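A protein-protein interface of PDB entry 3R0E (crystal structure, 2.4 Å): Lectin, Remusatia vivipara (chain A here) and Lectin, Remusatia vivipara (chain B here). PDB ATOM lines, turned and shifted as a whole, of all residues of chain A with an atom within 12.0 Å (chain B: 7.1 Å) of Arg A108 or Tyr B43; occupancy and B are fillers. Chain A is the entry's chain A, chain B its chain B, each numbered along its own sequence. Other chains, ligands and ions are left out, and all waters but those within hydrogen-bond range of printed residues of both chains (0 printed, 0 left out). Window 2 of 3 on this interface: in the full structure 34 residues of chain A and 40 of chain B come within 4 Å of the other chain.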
ATOM      1  N   PHE A 101      -5.005  -6.777  35.321  1.00  0.00           N
ATOM      2  CA  PHE A 101      -5.695  -8.068  35.226  1.00  0.00           C
ATOM      3  C   PHE A 101      -6.716  -8.016  34.103  1.00  0.00           C
ATOM      4  O   PHE A 101      -7.332  -6.975  33.852  1.00  0.00           O
ATOM      5  CB  PHE A 101      -6.405  -8.400  36.555  1.00  0.00           C
ATOM      6  CG  PHE A 101      -7.093  -9.743  36.578  1.00  0.00           C
ATOM      7  CD1 PHE A 101      -6.352 -10.930  36.607  1.00  0.00           C
ATOM      8  CD2 PHE A 101      -8.485  -9.823  36.612  1.00  0.00           C
ATOM      9  CE1 PHE A 101      -6.986 -12.181  36.644  1.00  0.00           C
ATOM     10  CE2 PHE A 101      -9.133 -11.067  36.650  1.00  0.00           C
ATOM     11  CZ  PHE A 101      -8.382 -12.246  36.668  1.00  0.00           C
ATOM     12  N   LYS A 102      -6.893  -9.147  33.437  1.00  0.00           N
ATOM     13  CA  LYS A 102      -7.826  -9.256  32.337  1.00  0.00           C
ATOM     14  C   LYS A 102      -8.616 -10.557  32.443  1.00  0.00           C
ATOM     15  O   LYS A 102      -8.035 -11.635  32.606  1.00  0.00           O
ATOM     16  CB  LYS A 102      -7.071  -9.176  31.003  1.00  0.00           C
ATOM     17  CG  LYS A 102      -7.922  -9.463  29.772  1.00  0.00           C
ATOM     18  CD  LYS A 102      -7.108  -9.415  28.472  1.00  0.00           C
ATOM     19  CE  LYS A 102      -7.010  -7.986  27.917  1.00  0.00           C
ATOM     20  NZ  LYS A 102      -6.490  -7.927  26.508  1.00  0.00           N
ATOM     21  N   ILE A 103      -9.942 -10.439  32.383  1.00  0.00           N
ATOM     22  CA  ILE A 103     -10.838 -11.586  32.176  1.00  0.00           C
ATOM     23  C   ILE A 103     -11.177 -11.671  30.688  1.00  0.00           C
ATOM     24  O   ILE A 103     -11.690 -10.719  30.095  1.00  0.00           O
ATOM     25  CB  ILE A 103     -12.130 -11.472  32.996  1.00  0.00           C
ATOM     26  CG1 ILE A 103     -11.827 -11.540  34.490  1.00  0.00           C
ATOM     27  CG2 ILE A 103     -13.099 -12.582  32.622  1.00  0.00           C
ATOM     28  CD1 ILE A 103     -12.971 -11.060  35.368  1.00  0.00           C
ATOM     29  N   ASP A 104     -10.879 -12.828  30.103  1.00  0.00           N
ATOM     30  CA  ASP A 104     -10.881 -13.015  28.657  1.00  0.00           C
ATOM     31  C   ASP A 104     -11.840 -14.138  28.268  1.00  0.00           C
ATOM     32  O   ASP A 104     -11.555 -15.315  28.513  1.00  0.00           O
ATOM     33  CB  ASP A 104      -9.453 -13.346  28.189  1.00  0.00           C
ATOM     34  CG  ASP A 104      -9.303 -13.336  26.681  1.00  0.00           C
ATOM     35  OD1 ASP A 104     -10.314 -13.514  25.962  1.00  0.00           O
ATOM     36  OD2 ASP A 104      -8.154 -13.156  26.206  1.00  0.00           O
ATOM     37  N   PRO A 105     -12.982 -13.779  27.664  1.00  0.00           N
ATOM     38  CA  PRO A 105     -13.968 -14.768  27.245  1.00  0.00           C
ATOM     39  C   PRO A 105     -13.712 -15.305  25.833  1.00  0.00           C
ATOM     40  O   PRO A 105     -14.513 -16.093  25.325  1.00  0.00           O
ATOM     41  CB  PRO A 105     -15.271 -13.969  27.276  1.00  0.00           C
ATOM     42  CG  PRO A 105     -14.857 -12.615  26.876  1.00  0.00           C
ATOM     43  CD  PRO A 105     -13.471 -12.406  27.451  1.00  0.00           C
ATOM     44  N   TRP A 106     -12.603 -14.888  25.223  1.00  0.00           N
ATOM     45  CA  TRP A 106     -12.294 -15.221  23.836  1.00  0.00           C
ATOM     46  C   TRP A 106     -11.237 -16.315  23.661  1.00  0.00           C
ATOM     47  O   TRP A 106     -10.959 -16.732  22.544  1.00  0.00           O
ATOM     48  CB  TRP A 106     -11.866 -13.961  23.076  1.00  0.00           C
ATOM     49  CG  TRP A 106     -12.881 -12.864  23.119  1.00  0.00           C
ATOM     50  CD1 TRP A 106     -12.873 -11.767  23.938  1.00  0.00           C
ATOM     51  CD2 TRP A 106     -14.063 -12.755  22.319  1.00  0.00           C
ATOM     52  NE1 TRP A 106     -13.974 -10.980  23.694  1.00  0.00           N
ATOM     53  CE2 TRP A 106     -14.725 -11.563  22.709  1.00  0.00           C
ATOM     54  CE3 TRP A 106     -14.630 -13.547  21.310  1.00  0.00           C
ATOM     55  CZ2 TRP A 106     -15.918 -11.138  22.120  1.00  0.00           C
ATOM     56  CZ3 TRP A 106     -15.823 -13.122  20.724  1.00  0.00           C
ATOM     57  CH2 TRP A 106     -16.450 -11.925  21.131  1.00  0.00           C
ATOM     58  N   VAL A 107     -10.638 -16.778  24.751  1.00  0.00           N
ATOM     59  CA  VAL A 107      -9.624 -17.827  24.665  1.00  0.00           C
ATOM     60  C   VAL A 107      -9.933 -18.950  25.639  1.00  0.00           C
ATOM     61  O   VAL A 107     -10.580 -18.724  26.666  1.00  0.00           O
ATOM     62  CB  VAL A 107      -8.183 -17.305  24.924  1.00  0.00           C
ATOM     63  CG1 VAL A 107      -7.745 -16.325  23.839  1.00  0.00           C
ATOM     64  CG2 VAL A 107      -8.060 -16.693  26.318  1.00  0.00           C
ATOM     65  N   ARG A 108      -9.471 -20.157  25.314  1.00  0.00           N
ATOM     66  CA  ARG A 108      -9.691 -21.319  26.170  1.00  0.00           C
ATOM     67  C   ARG A 108      -9.328 -20.967  27.616  1.00  0.00           C
ATOM     68  O   ARG A 108      -8.286 -20.355  27.868  1.00  0.00           O
ATOM     69  CB  ARG A 108      -8.871 -22.498  25.678  1.00  0.00           C
ATOM     70  N   GLY A 109     -10.209 -21.321  28.550  1.00  0.00           N
ATOM     71  CA  GLY A 109      -9.969 -21.093  29.974  1.00  0.00           C
ATOM     72  C   GLY A 109      -9.387 -22.323  30.648  1.00  0.00           C
ATOM     73  O   GLY A 109      -9.581 -22.530  31.846  1.00  0.00           O
ATOM     74  N   LEU B  38     -18.802 -14.456  33.314  1.00  0.00           N
ATOM     75  CA  LEU B  38     -18.865 -13.562  32.191  1.00  0.00           C
ATOM     76  C   LEU B  38     -19.588 -14.291  31.064  1.00  0.00           C
ATOM     77  O   LEU B  38     -19.076 -15.264  30.521  1.00  0.00           O
ATOM     78  CB  LEU B  38     -17.448 -13.118  31.787  1.00  0.00           C
ATOM     79  CG  LEU B  38     -17.102 -12.362  30.490  1.00  0.00           C
ATOM     80  CD1 LEU B  38     -18.259 -11.730  29.739  1.00  0.00           C
ATOM     81  CD2 LEU B  38     -16.031 -11.313  30.765  1.00  0.00           C
ATOM     82  N   GLY B  40     -21.091 -14.478  27.306  1.00  0.00           N
ATOM     83  CA  GLY B  40     -20.858 -13.942  25.974  1.00  0.00           C
ATOM     84  C   GLY B  40     -19.442 -14.219  25.523  1.00  0.00           C
ATOM     85  O   GLY B  40     -18.600 -14.647  26.314  1.00  0.00           O
ATOM     86  N   GLY B  41     -19.185 -13.969  24.243  1.00  0.00           N
ATOM     87  CA  GLY B  41     -17.907 -14.292  23.644  1.00  0.00           C
ATOM     88  C   GLY B  41     -17.834 -15.760  23.249  1.00  0.00           C
ATOM     89  O   GLY B  41     -18.762 -16.540  23.492  1.00  0.00           O
ATOM     90  N   LYS B  42     -16.707 -16.131  22.655  1.00  0.00           N
ATOM     91  CA  LYS B  42     -16.474 -17.466  22.147  1.00  0.00           C
ATOM     92  C   LYS B  42     -16.608 -18.516  23.247  1.00  0.00           C
ATOM     93  O   LYS B  42     -17.362 -19.479  23.088  1.00  0.00           O
ATOM     94  CB  LYS B  42     -15.096 -17.514  21.474  1.00  0.00           C
ATOM     95  CG  LYS B  42     -14.819 -18.725  20.617  1.00  0.00           C
ATOM     96  CD  LYS B  42     -13.723 -18.421  19.595  1.00  0.00           C
ATOM     97  CE  LYS B  42     -13.127 -19.691  19.030  1.00  0.00           C
ATOM     98  NZ  LYS B  42     -12.044 -19.419  18.041  1.00  0.00           N
ATOM     99  N   TYR B  43     -15.904 -18.315  24.362  1.00  0.00           N
ATOM    100  CA  TYR B  43     -15.851 -19.300  25.438  1.00  0.00           C
ATOM    101  C   TYR B  43     -16.574 -18.890  26.713  1.00  0.00           C
ATOM    102  O   TYR B  43     -16.890 -19.744  27.549  1.00  0.00           O
ATOM    103  CB  TYR B  43     -14.406 -19.583  25.823  1.00  0.00           C
ATOM    104  CG  TYR B  43     -13.578 -20.248  24.753  1.00  0.00           C
ATOM    105  CD1 TYR B  43     -13.451 -21.637  24.707  1.00  0.00           C
ATOM    106  CD2 TYR B  43     -12.902 -19.487  23.798  1.00  0.00           C
ATOM    107  CE1 TYR B  43     -12.670 -22.255  23.719  1.00  0.00           C
ATOM    108  CE2 TYR B  43     -12.121 -20.088  22.816  1.00  0.00           C
ATOM    109  CZ  TYR B  43     -12.012 -21.468  22.780  1.00  0.00           C
ATOM    110  OH  TYR B  43     -11.248 -22.051  21.805  1.00  0.00           O
ATOM    111  N   GLY B  44     -16.800 -17.590  26.892  1.00  0.00           N
ATOM    112  CA  GLY B  44     -17.214 -17.081  28.193  1.00  0.00           C
ATOM    113  C   GLY B  44     -16.077 -17.267  29.185  1.00  0.00           C
ATOM    114  O   GLY B  44     -14.956 -17.614  28.798  1.00  0.00           O
ATOM    115  N   TRP B  45     -16.366 -17.025  30.461  1.00  0.00           N
ATOM    116  CA  TRP B  45     -15.393 -17.173  31.536  1.00  0.00           C
ATOM    117  C   TRP B  45     -16.150 -17.358  32.837  1.00  0.00           C
ATOM    118  O   TRP B  45     -17.275 -16.874  32.993  1.00  0.00           O
ATOM    119  CB  TRP B  45     -14.483 -15.942  31.632  1.00  0.00           C
ATOM    120  CG  TRP B  45     -13.440 -16.028  32.728  1.00  0.00           C
ATOM    121  CD1 TRP B  45     -12.166 -16.514  32.613  1.00  0.00           C
ATOM    122  CD2 TRP B  45     -13.592 -15.626  34.103  1.00  0.00           C
ATOM    123  NE1 TRP B  45     -11.515 -16.446  33.828  1.00  0.00           N
ATOM    124  CE2 TRP B  45     -12.368 -15.906  34.759  1.00  0.00           C
ATOM    125  CE3 TRP B  45     -14.643 -15.063  34.843  1.00  0.00           C
ATOM    126  CZ2 TRP B  45     -12.165 -15.630  36.118  1.00  0.00           C
ATOM    127  CZ3 TRP B  45     -14.447 -14.796  36.191  1.00  0.00           C
ATOM    128  CH2 TRP B  45     -13.217 -15.082  36.817  1.00  0.00           C
ATOM    129  N   GLN B  46     -15.529 -18.063  33.773  1.00  0.00           N
ATOM    130  CA  GLN B  46     -16.123 -18.312  35.072  1.00  0.00           C
ATOM    131  C   GLN B  46     -15.022 -18.473  36.119  1.00  0.00           C
ATOM    132  O   GLN B  46     -14.012 -19.132  35.870  1.00  0.00           O
ATOM    133  CB  GLN B  46     -17.002 -19.573  35.022  1.00  0.00           C
ATOM    134  CG  GLN B  46     -16.251 -20.873  34.629  1.00  0.00           C
ATOM    135  CD  GLN B  46     -16.990 -22.162  35.017  1.00  0.00           C
ATOM    136  OE1 GLN B  46     -16.462 -23.268  34.840  1.00  0.00           O
ATOM    137  NE2 GLN B  46     -18.209 -22.025  35.548  1.00  0.00           N
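N of Val A107 is in hydrogen-bond range of OD1 of Asp A104, at 3.5 Å.
The backbone NH of Leu B38 is in hydrogen-bond range of the backbone carbonyl oxygen of Trp B45 (2.9 Å).
OD1 of Asp A104 sits at hydrogen-bond distance from N of Trp A106 (2.8 Å).
Arg A108 touches just one residue of chain B: Tyr B43 (3.6 Å).
Tyr B43 touches just these residues of chain A: Pro A105 (2.8 Å), Trp A106 (3.6 Å), Val A107 (3.5 Å) and Arg A108 (3.6 Å).
Gly B41 touches just these residues of chain A: Pro A105 and Trp A106.
Printed residues of chain B within 4 Å of Pro A105: Gly B40, Gly B41, Lys B42, Tyr B43 and Gly B44.
Printed residues of chain B within 4 Å of Val A107: Tyr B43 (3.5 Å).
The nearest residue of chain B that does not touch Arg A108 is Gly B44 (6.7 Å).
The nearest residue of chain A that does not touch Tyr B43 is Gly A109 (5.0 Å).
Among the printed residues, merely in contact across the chains: Ile A103 with Leu B38 (3.7 Å), Ile A103 with Trp B45 (3.4 Å), Pro A105 with Gly B40 (3.5 Å), Pro A105 with Gly B41 (3.9 Å), Trp A106 with Gly B41 (3.7 Å), Trp A106 with Lys B42 (3.6 Å), Trp A106 with Tyr B43 (3.6 Å), Val A107 with Tyr B43 (3.5 Å) and Arg A108 with Tyr B43 (3.6 Å).
The backbone NH (N) of Lys B42 is in hydrogen-bond range of the backbone carbonyl oxygen (O) of Pro A105, 3.5 Å away.
The backbone carbonyl oxygen (O) of Pro A105 is in hydrogen-bond range of the backbone NH (N) of Gly B44, 3.2 Å away.
The backbone carbonyl oxygen (O) of Pro A105 sits at hydrogen-bond distance from the backbone NH (N) of Tyr B43 (2.8 Å).
Of the 8 printed residues of chain B, 7 touch a printed residue of chain A.
Of the 9 printed residues of chain A, 5 touch a printed residue of chain B.
Printed residues of chain A that touch a printed residue of chain B: Ile A103, Pro A105, Trp A106, Val A107 and Arg A108.
Along chain A the printed residues that touch a printed residue of chain B span positions 103 to 108.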
